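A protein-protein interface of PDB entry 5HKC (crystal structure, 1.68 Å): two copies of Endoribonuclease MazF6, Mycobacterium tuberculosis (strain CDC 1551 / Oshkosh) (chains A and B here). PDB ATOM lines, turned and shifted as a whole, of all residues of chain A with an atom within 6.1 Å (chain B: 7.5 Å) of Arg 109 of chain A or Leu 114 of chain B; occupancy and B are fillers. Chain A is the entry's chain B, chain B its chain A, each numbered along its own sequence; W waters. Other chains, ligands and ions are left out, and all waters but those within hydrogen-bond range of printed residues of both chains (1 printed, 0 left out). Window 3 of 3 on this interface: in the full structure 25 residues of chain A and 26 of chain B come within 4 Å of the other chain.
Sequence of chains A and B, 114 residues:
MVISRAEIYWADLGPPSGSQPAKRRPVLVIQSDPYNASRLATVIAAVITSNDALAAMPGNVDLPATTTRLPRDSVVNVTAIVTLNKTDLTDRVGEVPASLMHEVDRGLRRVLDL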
ATOM      1  N   ARG A   5      25.069 -42.684  -1.344  1.00  0.00           N
ATOM      2  CA  ARG A   5      25.041 -41.362  -0.740  1.00  0.00           C
ATOM      3  C   ARG A   5      26.033 -41.296   0.415  1.00  0.00           C
ATOM      4  O   ARG A   5      26.251 -42.285   1.123  1.00  0.00           O
ATOM      5  CB  ARG A   5      23.628 -41.021  -0.266  1.00  0.00           C
ATOM      6  CG  ARG A   5      23.434 -39.561   0.067  1.00  0.00           C
ATOM      7  CD  ARG A   5      21.994 -39.261   0.450  1.00  0.00           C
ATOM      8  NE  ARG A   5      21.724 -37.826   0.448  1.00  0.00           N
ATOM      9  CZ  ARG A   5      21.888 -37.022   1.495  1.00  0.00           C
ATOM     10  NH1 ARG A   5      22.353 -37.495   2.649  1.00  0.00           N
ATOM     11  NH2 ARG A   5      21.608 -35.730   1.383  1.00  0.00           N
ATOM     12  N   HIS A 102      24.566 -35.177   8.418  1.00  0.00           N
ATOM     13  CA  HIS A 102      23.397 -34.441   8.904  1.00  0.00           C
ATOM     14  C   HIS A 102      23.615 -32.939   8.773  1.00  0.00           C
ATOM     15  O   HIS A 102      22.676 -32.187   8.511  1.00  0.00           O
ATOM     16  CB  HIS A 102      23.086 -34.808  10.351  1.00  0.00           C
ATOM     17  CG  HIS A 102      22.615 -36.219  10.525  1.00  0.00           C
ATOM     18  ND1 HIS A 102      22.709 -36.897  11.719  1.00  0.00           N
ATOM     19  CD2 HIS A 102      22.038 -37.079   9.647  1.00  0.00           C
ATOM     20  CE1 HIS A 102      22.214 -38.115  11.575  1.00  0.00           C
ATOM     21  NE2 HIS A 102      21.802 -38.248  10.325  1.00  0.00           N
ATOM     22  N   VAL A 104      25.591 -31.594   6.487  1.00  0.00           N
ATOM     23  CA  VAL A 104      25.485 -31.349   5.049  1.00  0.00           C
ATOM     24  C   VAL A 104      24.004 -31.260   4.637  1.00  0.00           C
ATOM     25  O   VAL A 104      23.623 -30.358   3.887  1.00  0.00           O
ATOM     26  CB  VAL A 104      26.206 -32.440   4.227  1.00  0.00           C
ATOM     27  CG1 VAL A 104      25.975 -32.227   2.740  1.00  0.00           C
ATOM     28  CG2 VAL A 104      27.706 -32.430   4.518  1.00  0.00           C
ATOM     29  N   ASP A 105      23.175 -32.178   5.136  1.00  0.00           N
ATOM     30  CA  ASP A 105      21.736 -32.160   4.828  1.00  0.00           C
ATOM     31  C   ASP A 105      21.132 -30.818   5.186  1.00  0.00           C
ATOM     32  O   ASP A 105      20.340 -30.255   4.437  1.00  0.00           O
ATOM     33  CB  ASP A 105      20.963 -33.249   5.591  1.00  0.00           C
ATOM     34  CG  ASP A 105      21.331 -34.648   5.167  1.00  0.00           C
ATOM     35  OD1 ASP A 105      21.982 -34.806   4.115  1.00  0.00           O
ATOM     36  OD2 ASP A 105      20.957 -35.598   5.898  1.00  0.00           O
ATOM     37  N   ARG A 106      21.502 -30.322   6.360  1.00  0.00           N
ATOM     38  CA  ARG A 106      20.977 -29.066   6.855  1.00  0.00           C
ATOM     39  C   ARG A 106      21.409 -27.926   5.952  1.00  0.00           C
ATOM     40  O   ARG A 106      20.620 -27.025   5.652  1.00  0.00           O
ATOM     41  CB  ARG A 106      21.447 -28.835   8.297  1.00  0.00           C
ATOM     42  CG  ARG A 106      20.650 -27.801   9.057  1.00  0.00           C
ATOM     43  CD  ARG A 106      21.040 -27.867  10.539  1.00  0.00           C
ATOM     44  NE  ARG A 106      22.453 -27.544  10.674  1.00  0.00           N
ATOM     45  CZ  ARG A 106      23.343 -28.280  11.322  1.00  0.00           C
ATOM     46  NH1 ARG A 106      22.979 -29.395  11.937  1.00  0.00           N
ATOM     47  NH2 ARG A 106      24.608 -27.874  11.368  1.00  0.00           N
ATOM     48  N   GLY A 107      22.658 -27.989   5.497  1.00  0.00           N
ATOM     49  CA  GLY A 107      23.189 -26.980   4.591  1.00  0.00           C
ATOM     50  C   GLY A 107      22.467 -27.000   3.251  1.00  0.00           C
ATOM     51  O   GLY A 107      22.122 -25.958   2.706  1.00  0.00           O
ATOM     52  N   LEU A 108      22.229 -28.194   2.728  1.00  0.00           N
ATOM     53  CA  LEU A 108      21.492 -28.332   1.473  1.00  0.00           C
ATOM     54  C   LEU A 108      20.059 -27.826   1.579  1.00  0.00           C
ATOM     55  O   LEU A 108      19.557 -27.158   0.680  1.00  0.00           O
ATOM     56  CB  LEU A 108      21.492 -29.789   1.036  1.00  0.00           C
ATOM     57  CG  LEU A 108      22.863 -30.359   0.681  1.00  0.00           C
ATOM     58  CD1 LEU A 108      22.775 -31.880   0.574  1.00  0.00           C
ATOM     59  CD2 LEU A 108      23.401 -29.757  -0.633  1.00  0.00           C
ATOM     60  N   ARG A 109      19.396 -28.160   2.678  1.00  0.00           N
ATOM     61  CA  ARG A 109      18.028 -27.700   2.862  1.00  0.00           C
ATOM     62  C   ARG A 109      18.003 -26.174   2.921  1.00  0.00           C
ATOM     63  O   ARG A 109      17.105 -25.540   2.386  1.00  0.00           O
ATOM     64  CB  ARG A 109      17.414 -28.344   4.114  1.00  0.00           C
ATOM     65  CG  ARG A 109      16.863 -29.765   3.837  1.00  0.00           C
ATOM     66  CD  ARG A 109      16.044 -30.318   5.024  1.00  0.00           C
ATOM     67  NE  ARG A 109      16.892 -30.497   6.195  1.00  0.00           N
ATOM     68  CZ  ARG A 109      17.447 -31.652   6.543  1.00  0.00           C
ATOM     69  NH1 ARG A 109      17.194 -32.762   5.845  1.00  0.00           N
ATOM     70  NH2 ARG A 109      18.237 -31.710   7.605  1.00  0.00           N
ATOM     71  N   ARG A 110      19.021 -25.578   3.538  1.00  0.00           N
ATOM     72  CA  ARG A 110      19.103 -24.128   3.601  1.00  0.00           C
ATOM     73  C   ARG A 110      19.310 -23.498   2.221  1.00  0.00           C
ATOM     74  O   ARG A 110      18.629 -22.548   1.852  1.00  0.00           O
ATOM     75  CB  ARG A 110      20.227 -23.699   4.543  1.00  0.00           C
ATOM     76  CG  ARG A 110      20.322 -22.202   4.751  1.00  0.00           C
ATOM     77  CD  ARG A 110      21.488 -21.871   5.667  1.00  0.00           C
ATOM     78  NE  ARG A 110      21.630 -20.432   5.853  1.00  0.00           N
ATOM     79  CZ  ARG A 110      22.388 -19.876   6.790  1.00  0.00           C
ATOM     80  NH1 ARG A 110      23.100 -20.648   7.603  1.00  0.00           N
ATOM     81  NH2 ARG A 110      22.465 -18.555   6.886  1.00  0.00           N
ATOM     82  N   VAL A 111      20.266 -24.018   1.458  1.00  0.00           N
ATOM     83  CA  VAL A 111      20.587 -23.401   0.164  1.00  0.00           C
ATOM     84  C   VAL A 111      19.484 -23.597  -0.859  1.00  0.00           C
ATOM     85  O   VAL A 111      19.340 -22.790  -1.772  1.00  0.00           O
ATOM     86  CB  VAL A 111      21.907 -23.948  -0.438  1.00  0.00           C
ATOM     87  CG1 VAL A 111      23.027 -23.792   0.552  1.00  0.00           C
ATOM     88  CG2 VAL A 111      21.766 -25.381  -0.914  1.00  0.00           C
ATOM     89  N   LEU A 112      18.685 -24.651  -0.688  1.00  0.00           N
ATOM     90  CA  LEU A 112      17.622 -24.958  -1.642  1.00  0.00           C
ATOM     91  C   LEU A 112      16.226 -24.625  -1.121  1.00  0.00           C
ATOM     92  O   LEU A 112      15.242 -24.898  -1.800  1.00  0.00           O
ATOM     93  CB  LEU A 112      17.675 -26.437  -2.037  1.00  0.00           C
ATOM     94  CG  LEU A 112      18.970 -26.946  -2.680  1.00  0.00           C
ATOM     95  CD1 LEU A 112      18.842 -28.447  -2.883  1.00  0.00           C
ATOM     96  CD2 LEU A 112      19.189 -26.242  -4.011  1.00  0.00           C
ATOM     97  N   ASP A 113      16.156 -24.014   0.064  1.00  0.00           N
ATOM     98  CA  ASP A 113      14.871 -23.641   0.673  1.00  0.00           C
ATOM     99  C   ASP A 113      13.933 -24.842   0.808  1.00  0.00           C
ATOM    100  O   ASP A 113      12.750 -24.755   0.469  1.00  0.00           O
ATOM    101  CB  ASP A 113      14.179 -22.536  -0.135  1.00  0.00           C
ATOM    102  CG  ASP A 113      13.132 -21.777   0.680  1.00  0.00           C
ATOM    103  OD1 ASP A 113      12.866 -22.171   1.843  1.00  0.00           O
ATOM    104  OD2 ASP A 113      12.593 -20.780   0.141  1.00  0.00           O
ATOM    105  N   LEU A 114      14.469 -25.956   1.303  1.00  0.00           N
ATOM    106  CA  LEU A 114      13.698 -27.181   1.486  1.00  0.00           C
ATOM    107  C   LEU A 114      13.489 -27.501   2.964  1.00  0.00           C
ATOM    108  O   LEU A 114      14.007 -26.796   3.809  1.00  0.00           O
ATOM    109  CB  LEU A 114      14.389 -28.358   0.812  1.00  0.00           C
ATOM    110  CG  LEU A 114      14.605 -28.239  -0.701  1.00  0.00           C
ATOM    111  CD1 LEU A 114      15.512 -29.367  -1.220  1.00  0.00           C
ATOM    112  CD2 LEU A 114      13.273 -28.215  -1.447  1.00  0.00           C
ATOM    113  N   ARG B   5      13.912 -17.532  -6.518  1.00  0.00           N
ATOM    114  CA  ARG B   5      13.542 -18.941  -6.550  1.00  0.00           C
ATOM    115  C   ARG B   5      12.200 -19.076  -7.268  1.00  0.00           C
ATOM    116  O   ARG B   5      11.344 -18.177  -7.158  1.00  0.00           O
ATOM    117  CB  ARG B   5      13.462 -19.522  -5.128  1.00  0.00           C
ATOM    118  CG  ARG B   5      13.386 -21.050  -5.104  1.00  0.00           C
ATOM    119  CD  ARG B   5      13.414 -21.604  -3.693  1.00  0.00           C
ATOM    120  NE  ARG B   5      13.717 -23.039  -3.682  1.00  0.00           N
ATOM    121  CZ  ARG B   5      12.807 -24.007  -3.710  1.00  0.00           C
ATOM    122  NH1 ARG B   5      11.519 -23.711  -3.743  1.00  0.00           N
ATOM    123  NH2 ARG B   5      13.188 -25.284  -3.696  1.00  0.00           N
ATOM    124  N   ILE B  30      16.220 -23.071  -8.141  1.00  0.00           N
ATOM    125  CA  ILE B  30      15.818 -23.721  -6.899  1.00  0.00           C
ATOM    126  C   ILE B  30      16.641 -23.239  -5.706  1.00  0.00           C
ATOM    127  O   ILE B  30      16.370 -23.596  -4.572  1.00  0.00           O
ATOM    128  CB  ILE B  30      15.905 -25.270  -7.008  1.00  0.00           C
ATOM    129  CG1 ILE B  30      17.313 -25.748  -7.398  1.00  0.00           C
ATOM    130  CG2 ILE B  30      14.901 -25.781  -8.034  1.00  0.00           C
ATOM    131  CD1 ILE B  30      17.479 -27.258  -7.262  1.00  0.00           C
ATOM    132  N   SER B  32      17.717 -20.776  -2.774  1.00  0.00           N
ATOM    133  CA  SER B  32      16.876 -19.914  -1.942  1.00  0.00           C
ATOM    134  C   SER B  32      17.242 -18.433  -2.130  1.00  0.00           C
ATOM    135  O   SER B  32      18.380 -18.077  -2.452  1.00  0.00           O
ATOM    136  CB  SER B  32      16.982 -20.301  -0.460  1.00  0.00           C
ATOM    137  OG  SER B  32      18.277 -20.026   0.028  1.00  0.00           O
ATOM    138  N   TYR B  35      20.466 -16.575  -0.711  1.00  0.00           N
ATOM    139  CA  TYR B  35      21.671 -16.830  -1.494  1.00  0.00           C
ATOM    140  C   TYR B  35      21.627 -16.112  -2.844  1.00  0.00           C
ATOM    141  O   TYR B  35      22.648 -15.614  -3.332  1.00  0.00           O
ATOM    142  CB  TYR B  35      21.888 -18.339  -1.694  1.00  0.00           C
ATOM    143  CG  TYR B  35      22.251 -19.056  -0.407  1.00  0.00           C
ATOM    144  CD1 TYR B  35      21.264 -19.534   0.442  1.00  0.00           C
ATOM    145  CD2 TYR B  35      23.579 -19.221  -0.028  1.00  0.00           C
ATOM    146  CE1 TYR B  35      21.589 -20.187   1.622  1.00  0.00           C
ATOM    147  CE2 TYR B  35      23.914 -19.866   1.150  1.00  0.00           C
ATOM    148  CZ  TYR B  35      22.916 -20.345   1.975  1.00  0.00           C
ATOM    149  OH  TYR B  35      23.235 -20.987   3.153  1.00  0.00           O
ATOM    150  N   ASP B 105       9.574 -29.014  -4.751  1.00  0.00           N
ATOM    151  CA  ASP B 105      10.222 -29.171  -3.447  1.00  0.00           C
ATOM    152  C   ASP B 105      10.183 -30.620  -2.963  1.00  0.00           C
ATOM    153  O   ASP B 105      11.179 -31.166  -2.492  1.00  0.00           O
ATOM    154  CB  ASP B 105       9.559 -28.282  -2.386  1.00  0.00           C
ATOM    155  CG  ASP B 105       9.738 -26.809  -2.652  1.00  0.00           C
ATOM    156  OD1 ASP B 105      10.579 -26.442  -3.495  1.00  0.00           O
ATOM    157  OD2 ASP B 105       9.027 -26.011  -1.999  1.00  0.00           O
ATOM    158  N   LEU B 108      12.651 -32.716  -5.057  1.00  0.00           N
ATOM    159  CA  LEU B 108      14.036 -32.491  -4.664  1.00  0.00           C
ATOM    160  C   LEU B 108      14.358 -33.201  -3.343  1.00  0.00           C
ATOM    161  O   LEU B 108      15.425 -33.789  -3.193  1.00  0.00           O
ATOM    162  CB  LEU B 108      14.313 -30.994  -4.518  1.00  0.00           C
ATOM    163  CG  LEU B 108      14.235 -30.181  -5.803  1.00  0.00           C
ATOM    164  CD1 LEU B 108      14.247 -28.685  -5.475  1.00  0.00           C
ATOM    165  CD2 LEU B 108      15.375 -30.554  -6.746  1.00  0.00           C
ATOM    166  N   ARG B 109      13.452 -33.146  -2.374  1.00  0.00           N
ATOM    167  CA  ARG B 109      13.739 -33.865  -1.125  1.00  0.00           C
ATOM    168  C   ARG B 109      13.845 -35.369  -1.384  1.00  0.00           C
ATOM    169  O   ARG B 109      14.677 -36.060  -0.796  1.00  0.00           O
ATOM    170  CB  ARG B 109      12.681 -33.568  -0.052  1.00  0.00           C
ATOM    171  CG  ARG B 109      12.962 -32.231   0.634  1.00  0.00           C
ATOM    172  CD  ARG B 109      12.143 -32.054   1.919  1.00  0.00           C
ATOM    173  NE  ARG B 109      10.730 -32.132   1.601  1.00  0.00           N
ATOM    174  CZ  ARG B 109       9.953 -31.091   1.342  1.00  0.00           C
ATOM    175  NH1 ARG B 109      10.440 -29.857   1.382  1.00  0.00           N
ATOM    176  NH2 ARG B 109       8.675 -31.291   1.049  1.00  0.00           N
ATOM    177  N   ARG B 110      13.026 -35.879  -2.295  1.00  0.00           N
ATOM    178  CA  ARG B 110      13.087 -37.296  -2.607  1.00  0.00           C
ATOM    179  C   ARG B 110      14.416 -37.675  -3.280  1.00  0.00           C
ATOM    180  O   ARG B 110      15.063 -38.646  -2.880  1.00  0.00           O
ATOM    181  CB  ARG B 110      11.905 -37.691  -3.488  1.00  0.00           C
ATOM    182  CG  ARG B 110      11.805 -39.177  -3.747  1.00  0.00           C
ATOM    183  CD  ARG B 110      10.627 -39.499  -4.644  1.00  0.00           C
ATOM    184  NE  ARG B 110      10.560 -40.932  -4.902  1.00  0.00           N
ATOM    185  CZ  ARG B 110       9.480 -41.563  -5.348  1.00  0.00           C
ATOM    186  NH1 ARG B 110       8.361 -40.890  -5.581  1.00  0.00           N
ATOM    187  NH2 ARG B 110       9.519 -42.869  -5.548  1.00  0.00           N
ATOM    188  N   VAL B 111      14.820 -36.917  -4.297  1.00  0.00           N
ATOM    189  CA  VAL B 111      16.032 -37.269  -5.037  1.00  0.00           C
ATOM    190  C   VAL B 111      17.304 -37.012  -4.224  1.00  0.00           C
ATOM    191  O   VAL B 111      18.330 -37.658  -4.453  1.00  0.00           O
ATOM    192  CB  VAL B 111      16.110 -36.528  -6.397  1.00  0.00           C
ATOM    193  CG1 VAL B 111      14.842 -36.752  -7.165  1.00  0.00           C
ATOM    194  CG2 VAL B 111      16.384 -35.046  -6.230  1.00  0.00           C
ATOM    195  N   LEU B 112      17.244 -36.080  -3.266  1.00  0.00           N
ATOM    196  CA  LEU B 112      18.417 -35.764  -2.450  1.00  0.00           C
ATOM    197  C   LEU B 112      18.352 -36.312  -1.018  1.00  0.00           C
ATOM    198  O   LEU B 112      19.223 -36.032  -0.206  1.00  0.00           O
ATOM    199  CB  LEU B 112      18.620 -34.254  -2.398  1.00  0.00           C
ATOM    200  CG  LEU B 112      18.805 -33.547  -3.740  1.00  0.00           C
ATOM    201  CD1 LEU B 112      18.896 -32.047  -3.467  1.00  0.00           C
ATOM    202  CD2 LEU B 112      20.032 -34.064  -4.487  1.00  0.00           C
ATOM    203  N   ASP B 113      17.305 -37.072  -0.712  1.00  0.00           N
ATOM    204  CA  ASP B 113      17.126 -37.674   0.605  1.00  0.00           C
ATOM    205  C   ASP B 113      17.177 -36.595   1.700  1.00  0.00           C
ATOM    206  O   ASP B 113      17.901 -36.713   2.694  1.00  0.00           O
ATOM    207  CB  ASP B 113      18.185 -38.762   0.831  1.00  0.00           C
ATOM    208  CG  ASP B 113      17.741 -39.820   1.826  1.00  0.00           C
ATOM    209  OD1 ASP B 113      16.654 -39.671   2.423  1.00  0.00           O
ATOM    210  OD2 ASP B 113      18.469 -40.828   1.969  1.00  0.00           O
ATOM    211  N   LEU B 114      16.422 -35.522   1.496  1.00  0.00           N
ATOM    212  CA  LEU B 114      16.393 -34.430   2.469  1.00  0.00           C
ATOM    213  C   LEU B 114      15.040 -34.340   3.194  1.00  0.00           C
ATOM    214  O   LEU B 114      14.888 -33.528   4.118  1.00  0.00           O
ATOM    215  CB  LEU B 114      16.695 -33.099   1.796  1.00  0.00           C
ATOM    216  CG  LEU B 114      18.081 -33.019   1.134  1.00  0.00           C
ATOM    217  CD1 LEU B 114      18.207 -31.776   0.266  1.00  0.00           C
ATOM    218  CD2 LEU B 114      19.178 -33.066   2.199  1.00  0.00           C
HETATM  219  O   HOH W   1      10.060 -25.316   0.283  1.00  0.00           O
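The guanidinium group (NH2) of Arg 5 of chain B sits at hydrogen-bond distance from the backbone carbonyl oxygen (O) of Leu 112 of chain A (2.8 Å). The backbone NH of Ser 32 of chain B lies within hydrogen-bond range of the backbone carbonyl oxygen of Val 111 of chain A. The backbone carbonyl oxygen (O) of Leu 112 of chain B sits at hydrogen-bond distance from the guanidinium group (NH2) of Arg 5 of chain A (2.9 Å). The backbone carbonyl oxygen (O) of Ile 30 of chain B lies close to the backbone carbonyl oxygen (O) of Leu 112 of chain A (3.3 Å). OG of Ser 32 of chain B sits at hydrogen-bond distance from O of Arg 110 of chain A, at 3.1 Å. The guanidinium group of Arg 110 of chain A lies close to the side-chain hydroxyl of Tyr 35 of chain B (3.2 Å). The guanidinium group (NH1) of Arg 109 of chain A sits at hydrogen-bond distance from the backbone carbonyl oxygen (O) of Leu 114 of chain B (3.0 Å).
NE of Arg 5 of chain B is in hydrogen-bond range of O of Ile 30 of chain B, 2.9 Å away. N of Leu 114 of chain A lies within hydrogen-bond range of O of Arg 109 of chain A (2.9 Å). The guanidinium group (NH2) of Arg 5 of chain A lies within salt-bridge range of the side-chain carboxylate (OD1) of Asp 105 of chain A, 2.9 Å away. The guanidinium group of Arg 5 of chain B is in salt-bridge range of the side-chain carboxylate of Asp 105 of chain B. The backbone NH (N) of Leu 114 of chain B is in hydrogen-bond range of the backbone carbonyl oxygen (O) of Arg 109 of chain B, at 2.9 Å.
Among the printed residues, pairs that only touch across the chains: Arg 5 of chain A with Asp 113 of chain B (3.7 Å), Arg 5 of chain A with Leu 114 of chain B (3.7 Å), Asp 105 of chain A with Leu 114 of chain B (3.8 Å), Leu 108 of chain A with Leu 114 of chain B (3.9 Å), Val 111 of chain A with Tyr 35 of chain B (3.7 Å), Leu 112 of chain A with Leu 112 of chain B (3.6 Å), Asp 113 of chain A with Arg 5 of chain B (3.6 Å), Asp 113 of chain A with Ser 32 of chain B (3.6 Å), Leu 114 of chain A with Arg 5 of chain B (3.7 Å), Leu 114 of chain A with Asp 105 of chain B (3.8 Å), Leu 114 of chain A with Leu 108 of chain B (3.9 Å) and Leu 114 of chain A with Leu 114 of chain B (3.9 Å).
Of the printed residues of chain B, Asp 105 of chain A touches Leu 114. Printed residues of chain B within 4 Å of Leu 108 of chain A: Leu 114 (3.9 Å). Of the printed residues of chain A, Ile 30 of chain B touches Leu 112 (3.3 Å). Printed residues of chain A within 4 Å of Leu 108 of chain B: Leu 114. Arg 109 of chain B touches none of the printed residues of chain A. Arg 110 of chain B touches none of the printed residues of chain A. Of chain A, only Arg 5, Asp 105, Leu 108, Arg 109 and Leu 114 come within 4 Å of Leu 114 of chain B.
Of the 12 printed residues of chain B, 9 touch a printed residue of chain A. Hydrophobic or aromatic side chains of chain B within 4 Å of the printed part of chain A: Ile 30, Tyr 35, Leu 108, Leu 112 and Leu 114. Of the 13 printed residues of chain A, 9 touch a printed residue of chain B. Printed residues of chain A that touch a printed residue of chain B: Arg 5, Asp 105, Leu 108, Arg 109, Arg 110, Val 111, Leu 112, Asp 113 and Leu 114. Hydrophobic or aromatic side chains of chain A within 4 Å of the printed part of chain B: Leu 108, Val 111, Leu 112 and Leu 114. Among the printed residues, 19 pairs touch across the chains. Among the printed residues, no Asp or Glu carboxylate lies within 4 Å of a Lys or Arg side-chain nitrogen of the other chain.
Asp 105 of chain A touches Leu 114 of chain B, and with the chains exchanged Leu 114 of chain A touches Asp 105 of chain B. Leu 108 of chain A touches Leu 114 of chain B, and with the chains exchanged Leu 114 of chain A touches Leu 108 of chain B. Arg 109 of chain A touches Leu 114 of chain B, but with the chains exchanged Leu 114 of chain A does not touch Arg 109 of chain B (4.1 Å). Leu 114 of chain A touches its own counterpart, Leu 114 of chain B. Of the 19 pairs that touch across the chains among the printed residues, 12 have their exchanged pair printed and touching as well.
Water W1 lies within hydrogen-bond range of OD2 of Asp 105 of chain B (2.6 Å) and O of Asp 113 of chain A (2.8 Å).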
